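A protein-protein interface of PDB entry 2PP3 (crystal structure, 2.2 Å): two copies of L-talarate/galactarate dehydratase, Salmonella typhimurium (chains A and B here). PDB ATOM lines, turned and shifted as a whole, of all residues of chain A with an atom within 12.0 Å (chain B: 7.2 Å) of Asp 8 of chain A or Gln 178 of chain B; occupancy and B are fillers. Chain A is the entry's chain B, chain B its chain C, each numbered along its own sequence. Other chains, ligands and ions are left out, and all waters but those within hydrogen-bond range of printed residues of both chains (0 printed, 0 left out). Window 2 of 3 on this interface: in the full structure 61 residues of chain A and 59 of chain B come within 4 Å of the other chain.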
ATOM      1  N   SER A   4      21.764   0.709  12.800  1.00  0.00           N
ATOM      2  CA  SER A   4      21.733   2.165  13.140  1.00  0.00           C
ATOM      3  C   SER A   4      20.711   2.479  14.225  1.00  0.00           C
ATOM      4  O   SER A   4      19.609   1.935  14.224  1.00  0.00           O
ATOM      5  CB  SER A   4      21.407   2.994  11.899  1.00  0.00           C
ATOM      6  OG  SER A   4      21.319   4.371  12.232  1.00  0.00           O
ATOM      7  N   ALA A   5      21.078   3.374  15.138  1.00  0.00           N
ATOM      8  CA  ALA A   5      20.197   3.756  16.235  1.00  0.00           C
ATOM      9  C   ALA A   5      19.266   4.922  15.891  1.00  0.00           C
ATOM     10  O   ALA A   5      18.414   5.296  16.699  1.00  0.00           O
ATOM     11  CB  ALA A   5      21.028   4.096  17.470  1.00  0.00           C
ATOM     12  N   ASN A   6      19.425   5.497  14.703  1.00  0.00           N
ATOM     13  CA  ASN A   6      18.570   6.611  14.291  1.00  0.00           C
ATOM     14  C   ASN A   6      18.226   6.529  12.802  1.00  0.00           C
ATOM     15  O   ASN A   6      18.639   5.595  12.113  1.00  0.00           O
ATOM     16  CB  ASN A   6      19.256   7.949  14.608  1.00  0.00           C
ATOM     17  CG  ASN A   6      20.316   8.331  13.584  1.00  0.00           C
ATOM     18  OD1 ASN A   6      21.136   7.506  13.168  1.00  0.00           O
ATOM     19  ND2 ASN A   6      20.307   9.598  13.181  1.00  0.00           N
ATOM     20  N   SER A   7      17.459   7.501  12.314  1.00  0.00           N
ATOM     21  CA  SER A   7      17.058   7.541  10.906  1.00  0.00           C
ATOM     22  C   SER A   7      16.715   8.969  10.489  1.00  0.00           C
ATOM     23  O   SER A   7      16.767   9.887  11.308  1.00  0.00           O
ATOM     24  CB  SER A   7      15.840   6.639  10.673  1.00  0.00           C
ATOM     25  OG  SER A   7      14.695   7.142  11.340  1.00  0.00           O
ATOM     26  N   ASP A   8      16.365   9.152   9.216  1.00  0.00           N
ATOM     27  CA  ASP A   8      16.006  10.474   8.702  1.00  0.00           C
ATOM     28  C   ASP A   8      14.786  11.004   9.442  1.00  0.00           C
ATOM     29  O   ASP A   8      14.644  12.210   9.648  1.00  0.00           O
ATOM     30  CB  ASP A   8      15.698  10.412   7.202  1.00  0.00           C
ATOM     31  CG  ASP A   8      16.905  10.021   6.369  1.00  0.00           C
ATOM     32  OD1 ASP A   8      17.947  10.705   6.467  1.00  0.00           O
ATOM     33  OD2 ASP A   8      16.807   9.031   5.611  1.00  0.00           O
ATOM     34  N   ALA A   9      13.900  10.094   9.832  1.00  0.00           N
ATOM     35  CA  ALA A   9      12.696  10.469  10.559  1.00  0.00           C
ATOM     36  C   ALA A   9      12.881  10.112  12.032  1.00  0.00           C
ATOM     37  O   ALA A   9      14.003  10.107  12.544  1.00  0.00           O
ATOM     38  CB  ALA A   9      11.486   9.737   9.986  1.00  0.00           C
ATOM     39  N   VAL A  10      11.778   9.820  12.706  1.00  0.00           N
ATOM     40  CA  VAL A  10      11.816   9.447  14.112  1.00  0.00           C
ATOM     41  C   VAL A  10      11.171   8.065  14.245  1.00  0.00           C
ATOM     42  O   VAL A  10      10.180   7.770  13.577  1.00  0.00           O
ATOM     43  CB  VAL A  10      11.057  10.488  14.979  1.00  0.00           C
ATOM     44  CG1 VAL A  10       9.619  10.623  14.497  1.00  0.00           C
ATOM     45  CG2 VAL A  10      11.097  10.079  16.444  1.00  0.00           C
ATOM     46  N   THR A  11      11.743   7.219  15.097  1.00  0.00           N
ATOM     47  CA  THR A  11      11.223   5.870  15.294  1.00  0.00           C
ATOM     48  C   THR A  11      10.782   5.614  16.734  1.00  0.00           C
ATOM     49  O   THR A  11      11.342   6.170  17.681  1.00  0.00           O
ATOM     50  CB  THR A  11      12.278   4.807  14.904  1.00  0.00           C
ATOM     51  OG1 THR A  11      12.653   4.988  13.533  1.00  0.00           O
ATOM     52  CG2 THR A  11      11.722   3.400  15.080  1.00  0.00           C
ATOM     53  N   TYR A  12       9.773   4.761  16.879  1.00  0.00           N
ATOM     54  CA  TYR A  12       9.222   4.400  18.179  1.00  0.00           C
ATOM     55  C   TYR A  12       9.027   2.885  18.240  1.00  0.00           C
ATOM     56  O   TYR A  12       8.448   2.290  17.331  1.00  0.00           O
ATOM     57  CB  TYR A  12       7.872   5.098  18.390  1.00  0.00           C
ATOM     58  CG  TYR A  12       7.969   6.591  18.613  1.00  0.00           C
ATOM     59  CD1 TYR A  12       8.241   7.110  19.881  1.00  0.00           C
ATOM     60  CD2 TYR A  12       7.810   7.487  17.556  1.00  0.00           C
ATOM     61  CE1 TYR A  12       8.354   8.480  20.093  1.00  0.00           C
ATOM     62  CE2 TYR A  12       7.924   8.866  17.755  1.00  0.00           C
ATOM     63  CZ  TYR A  12       8.196   9.353  19.027  1.00  0.00           C
ATOM     64  OH  TYR A  12       8.325  10.708  19.232  1.00  0.00           O
ATOM     65  N   ALA B  41      23.228   6.236  11.738  1.00  0.00           N
ATOM     66  CA  ALA B  41      23.234   6.266  10.273  1.00  0.00           C
ATOM     67  C   ALA B  41      23.072   7.674   9.724  1.00  0.00           C
ATOM     68  O   ALA B  41      23.739   8.057   8.761  1.00  0.00           O
ATOM     69  CB  ALA B  41      22.123   5.370   9.724  1.00  0.00           C
ATOM     70  N   THR B  42      22.173   8.438  10.335  1.00  0.00           N
ATOM     71  CA  THR B  42      21.928   9.809   9.914  1.00  0.00           C
ATOM     72  C   THR B  42      22.628  10.779  10.865  1.00  0.00           C
ATOM     73  O   THR B  42      22.185  10.975  11.994  1.00  0.00           O
ATOM     74  CB  THR B  42      20.419  10.117   9.904  1.00  0.00           C
ATOM     75  OG1 THR B  42      19.762   9.250   8.967  1.00  0.00           O
ATOM     76  CG2 THR B  42      20.172  11.573   9.520  1.00  0.00           C
ATOM     77  N   PRO B  43      23.736  11.394  10.417  1.00  0.00           N
ATOM     78  CA  PRO B  43      24.488  12.345  11.244  1.00  0.00           C
ATOM     79  C   PRO B  43      23.568  13.426  11.811  1.00  0.00           C
ATOM     80  O   PRO B  43      22.768  14.020  11.086  1.00  0.00           O
ATOM     81  CB  PRO B  43      25.520  12.906  10.268  1.00  0.00           C
ATOM     82  CG  PRO B  43      25.773  11.745   9.353  1.00  0.00           C
ATOM     83  CD  PRO B  43      24.371  11.233   9.097  1.00  0.00           C
ATOM     84  N   SER B 168      14.594  13.912  19.221  1.00  0.00           N
ATOM     85  CA  SER B 168      15.209  13.299  18.042  1.00  0.00           C
ATOM     86  C   SER B 168      14.625  13.665  16.673  1.00  0.00           C
ATOM     87  O   SER B 168      15.308  13.531  15.660  1.00  0.00           O
ATOM     88  CB  SER B 168      15.222  11.773  18.192  1.00  0.00           C
ATOM     89  OG  SER B 168      13.908  11.251  18.251  1.00  0.00           O
ATOM     90  N   GLY B 169      13.381  14.131  16.627  1.00  0.00           N
ATOM     91  CA  GLY B 169      12.791  14.483  15.345  1.00  0.00           C
ATOM     92  C   GLY B 169      12.696  15.972  15.044  1.00  0.00           C
ATOM     93  O   GLY B 169      11.922  16.379  14.171  1.00  0.00           O
ATOM     94  N   HIS B 173      19.491  19.483  11.105  1.00  0.00           N
ATOM     95  CA  HIS B 173      19.943  18.836   9.878  1.00  0.00           C
ATOM     96  C   HIS B 173      18.723  18.268   9.149  1.00  0.00           C
ATOM     97  O   HIS B 173      18.842  17.706   8.064  1.00  0.00           O
ATOM     98  CB  HIS B 173      20.929  17.710  10.204  1.00  0.00           C
ATOM     99  CG  HIS B 173      20.327  16.589  10.995  1.00  0.00           C
ATOM    100  ND1 HIS B 173      19.561  15.598  10.419  1.00  0.00           N
ATOM    101  CD2 HIS B 173      20.349  16.323  12.322  1.00  0.00           C
ATOM    102  CE1 HIS B 173      19.138  14.769  11.357  1.00  0.00           C
ATOM    103  NE2 HIS B 173      19.604  15.186  12.521  1.00  0.00           N
ATOM    104  N   THR B 174      17.551  18.437   9.756  1.00  0.00           N
ATOM    105  CA  THR B 174      16.295  17.936   9.202  1.00  0.00           C
ATOM    106  C   THR B 174      15.463  19.018   8.505  1.00  0.00           C
ATOM    107  O   THR B 174      15.067  20.010   9.122  1.00  0.00           O
ATOM    108  CB  THR B 174      15.424  17.298  10.316  1.00  0.00           C
ATOM    109  OG1 THR B 174      16.179  16.285  10.994  1.00  0.00           O
ATOM    110  CG2 THR B 174      14.161  16.675   9.726  1.00  0.00           C
ATOM    111  N   PRO B 175      15.183  18.836   7.204  1.00  0.00           N
ATOM    112  CA  PRO B 175      14.387  19.819   6.460  1.00  0.00           C
ATOM    113  C   PRO B 175      13.017  20.020   7.097  1.00  0.00           C
ATOM    114  O   PRO B 175      12.425  19.075   7.615  1.00  0.00           O
ATOM    115  CB  PRO B 175      14.302  19.211   5.058  1.00  0.00           C
ATOM    116  CG  PRO B 175      14.456  17.735   5.305  1.00  0.00           C
ATOM    117  CD  PRO B 175      15.544  17.694   6.349  1.00  0.00           C
ATOM    118  N   LEU B 176      12.520  21.252   7.063  1.00  0.00           N
ATOM    119  CA  LEU B 176      11.228  21.570   7.659  1.00  0.00           C
ATOM    120  C   LEU B 176      10.122  20.552   7.361  1.00  0.00           C
ATOM    121  O   LEU B 176       9.351  20.190   8.253  1.00  0.00           O
ATOM    122  CB  LEU B 176      10.771  22.963   7.216  1.00  0.00           C
ATOM    123  CG  LEU B 176       9.423  23.405   7.791  1.00  0.00           C
ATOM    124  CD1 LEU B 176       9.424  23.238   9.304  1.00  0.00           C
ATOM    125  CD2 LEU B 176       9.152  24.847   7.415  1.00  0.00           C
ATOM    126  N   ASP B 177      10.046  20.090   6.116  1.00  0.00           N
ATOM    127  CA  ASP B 177       9.018  19.125   5.724  1.00  0.00           C
ATOM    128  C   ASP B 177       9.108  17.814   6.512  1.00  0.00           C
ATOM    129  O   ASP B 177       8.084  17.232   6.869  1.00  0.00           O
ATOM    130  CB  ASP B 177       9.092  18.841   4.213  1.00  0.00           C
ATOM    131  CG  ASP B 177      10.374  18.122   3.803  1.00  0.00           C
ATOM    132  OD1 ASP B 177      10.548  16.938   4.173  1.00  0.00           O
ATOM    133  OD2 ASP B 177      11.209  18.740   3.104  1.00  0.00           O
ATOM    134  N   GLN B 178      10.331  17.355   6.776  1.00  0.00           N
ATOM    135  CA  GLN B 178      10.551  16.123   7.530  1.00  0.00           C
ATOM    136  C   GLN B 178      10.228  16.320   9.006  1.00  0.00           C
ATOM    137  O   GLN B 178       9.690  15.423   9.659  1.00  0.00           O
ATOM    138  CB  GLN B 178      12.001  15.659   7.392  1.00  0.00           C
ATOM    139  CG  GLN B 178      12.205  14.551   6.384  1.00  0.00           C
ATOM    140  CD  GLN B 178      11.381  13.321   6.711  1.00  0.00           C
ATOM    141  OE1 GLN B 178      11.448  12.792   7.821  1.00  0.00           O
ATOM    142  NE2 GLN B 178      10.597  12.859   5.741  1.00  0.00           N
ATOM    143  N   VAL B 179      10.568  17.493   9.530  1.00  0.00           N
ATOM    144  CA  VAL B 179      10.300  17.798  10.927  1.00  0.00           C
ATOM    145  C   VAL B 179       8.799  17.683  11.170  1.00  0.00           C
ATOM    146  O   VAL B 179       8.361  17.113  12.174  1.00  0.00           O
ATOM    147  CB  VAL B 179      10.775  19.223  11.298  1.00  0.00           C
ATOM    148  CG1 VAL B 179      10.377  19.548  12.738  1.00  0.00           C
ATOM    149  CG2 VAL B 179      12.291  19.326  11.119  1.00  0.00           C
ATOM    150  N   LEU B 180       8.016  18.224  10.239  1.00  0.00           N
ATOM    151  CA  LEU B 180       6.562  18.166  10.341  1.00  0.00           C
ATOM    152  C   LEU B 180       6.081  16.716  10.222  1.00  0.00           C
ATOM    153  O   LEU B 180       5.102  16.326  10.861  1.00  0.00           O
ATOM    154  CB  LEU B 180       5.927  19.045   9.260  1.00  0.00           C
ATOM    155  CG  LEU B 180       6.167  20.544   9.475  1.00  0.00           C
ATOM    156  CD1 LEU B 180       5.620  21.345   8.310  1.00  0.00           C
ATOM    157  CD2 LEU B 180       5.504  20.968  10.771  1.00  0.00           C
ATOM    158  N   LYS B 181       6.776  15.919   9.412  1.00  0.00           N
ATOM    159  CA  LYS B 181       6.423  14.509   9.250  1.00  0.00           C
ATOM    160  C   LYS B 181       6.696  13.786  10.565  1.00  0.00           C
ATOM    161  O   LYS B 181       5.953  12.882  10.958  1.00  0.00           O
ATOM    162  CB  LYS B 181       7.247  13.848   8.137  1.00  0.00           C
ATOM    163  CG  LYS B 181       6.768  14.120   6.714  1.00  0.00           C
ATOM    164  CD  LYS B 181       7.487  13.204   5.722  1.00  0.00           C
ATOM    165  CE  LYS B 181       6.984  13.396   4.297  1.00  0.00           C
ATOM    166  NZ  LYS B 181       7.253  14.769   3.780  1.00  0.00           N
ATOM    167  N   ASN B 182       7.769  14.184  11.244  1.00  0.00           N
ATOM    168  CA  ASN B 182       8.116  13.565  12.516  1.00  0.00           C
ATOM    169  C   ASN B 182       7.107  13.944  13.596  1.00  0.00           C
ATOM    170  O   ASN B 182       6.809  13.143  14.485  1.00  0.00           O
ATOM    171  CB  ASN B 182       9.531  13.970  12.945  1.00  0.00           C
ATOM    172  CG  ASN B 182      10.597  13.500  11.964  1.00  0.00           C
ATOM    173  OD1 ASN B 182      10.457  12.444  11.341  1.00  0.00           O
ATOM    174  ND2 ASN B 182      11.674  14.273  11.833  1.00  0.00           N
ATOM    175  N   VAL B 183       6.569  15.158  13.518  1.00  0.00           N
ATOM    176  CA  VAL B 183       5.591  15.594  14.508  1.00  0.00           C
ATOM    177  C   VAL B 183       4.389  14.651  14.538  1.00  0.00           C
ATOM    178  O   VAL B 183       4.036  14.127  15.597  1.00  0.00           O
ATOM    179  CB  VAL B 183       5.093  17.029  14.229  1.00  0.00           C
ATOM    180  CG1 VAL B 183       3.931  17.364  15.158  1.00  0.00           C
ATOM    181  CG2 VAL B 183       6.228  18.017  14.433  1.00  0.00           C
ATOM    182  N   VAL B 184       3.763  14.435  13.383  1.00  0.00           N
ATOM    183  CA  VAL B 184       2.606  13.543  13.316  1.00  0.00           C
ATOM    184  C   VAL B 184       2.954  12.150  13.853  1.00  0.00           C
ATOM    185  O   VAL B 184       2.238  11.608  14.695  1.00  0.00           O
ATOM    186  CB  VAL B 184       2.059  13.419  11.866  1.00  0.00           C
ATOM    187  CG1 VAL B 184       3.149  12.944  10.920  1.00  0.00           C
ATOM    188  CG2 VAL B 184       0.880  12.450  11.839  1.00  0.00           C
ATOM    189  N   ILE B 185       4.057  11.580  13.372  1.00  0.00           N
ATOM    190  CA  ILE B 185       4.498  10.263  13.825  1.00  0.00           C
ATOM    191  C   ILE B 185       4.597  10.250  15.350  1.00  0.00           C
ATOM    192  O   ILE B 185       4.093   9.337  16.007  1.00  0.00           O
ATOM    193  CB  ILE B 185       5.892   9.900  13.239  1.00  0.00           C
ATOM    194  CG1 ILE B 185       5.783   9.687  11.728  1.00  0.00           C
ATOM    195  CG2 ILE B 185       6.450   8.654  13.923  1.00  0.00           C
ATOM    196  CD1 ILE B 185       7.087   9.270  11.068  1.00  0.00           C
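ND2 of Asn 6 of chain A is in hydrogen-bond range of O of Thr 42 of chain B, at 2.6 Å. The backbone NH (N) of Asp 8 of chain A lies within hydrogen-bond range of the side-chain hydroxyl (OG1) of Thr 42 of chain B (3.4 Å). The side-chain hydroxyl of Ser 4 of chain A lies within hydrogen-bond range of the backbone NH of Ala 41 of chain B (2.7 Å). The backbone NH (N) of Ala 41 of chain B lies within hydrogen-bond range of the side-chain amide oxygen (OD1) of Asn 6 of chain A (2.8 Å). The backbone NH (N) of Val 10 of chain A sits at hydrogen-bond distance from the side-chain amide oxygen (OD1) of Asn 182 of chain B (3.2 Å).
O of Asn 6 of chain A is in hydrogen-bond range of OG of Ser 4 of chain A (2.9 Å). The backbone carbonyl oxygen of Gly 169 of chain B is in hydrogen-bond range of the side-chain amide nitrogen of Asn 182 of chain B (3.2 Å). O of Ala 9 of chain A sits at hydrogen-bond distance from OG of Ser 7 of chain A. The backbone carbonyl oxygen of Gln 178 of chain B sits close to the side-chain amide nitrogen of Asn 182 of chain B.
Ser 7 of chain A touches Thr 42 of chain B (C to OG1, 3.4 Å). Gln 178 of chain B touches Asp 8 of chain A. CB of Ala 9 of chain A touches OE1 of Gln 178 of chain B (3.7 Å). Ala 9 of chain A touches Asn 182 of chain B. Val 10 of chain A touches Ser 168 of chain B. Val 10 of chain A touches Ile 185 of chain B.
Of chain B, only Thr 42 (3.4 Å) and Gln 178 (3.7 Å) come within 4 Å of Asp 8 of chain A. Gln 178 of chain B touches just these residues of chain A: Asp 8 (3.7 Å) and Ala 9 (3.7 Å). Printed residues of chain A within 4 Å of Thr 42 of chain B: Asn 6 (2.6 Å), Ser 7 (3.4 Å) and Asp 8 (3.4 Å). No residue of chain A comes within 4 Å of Gly 169 of chain B. No residue of chain A comes within 4 Å of Pro 175 of chain B. No residue of chain A comes within 4 Å of Leu 176 of chain B. No residue of chain A comes within 4 Å of Val 179 of chain B. Leu 180 of chain B touches none of the printed residues of chain A. No residue of chain A comes within 4 Å of Lys 181 of chain B. Of chain A, only Ala 9 and Val 10 come within 4 Å of Asn 182 of chain B. Printed residues of chain A within 4 Å of Ile 185 of chain B: Val 10 (3.8 Å). Of the printed residues of chain B, Ser 7 of chain A touches Thr 42 (3.4 Å). Printed residues of chain B within 4 Å of Asn 6 of chain A: Ala 41 and Thr 42. Val 184 of chain B touches none of the printed residues of chain A. Tyr 12 of chain A touches none of the printed residues of chain B. The nearest printed residue of chain A that does not touch Ser 168 of chain B is Ala 9 of chain A (4.8 Å).
Printed residues of chain A that touch a printed residue of chain B: Ser 4, Asn 6, Ser 7, Asp 8, Ala 9 and Val 10. Hydrophobic or aromatic side chains of chain A within 4 Å of the printed part of chain B: Ala 9 and Val 10. Printed residues of chain B that touch a printed residue of chain A: Ala 41, Thr 42, Ser 168, Gln 178, Asn 182 and Ile 185. Among the printed residues, no Asp or Glu carboxylate lies within 4 Å of a Lys or Arg side-chain nitrogen of the other chain.
No position is printed for both chains. Of the 11 pairs that touch across the chains among the printed residues, none has its exchanged pair printed and touching as well.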
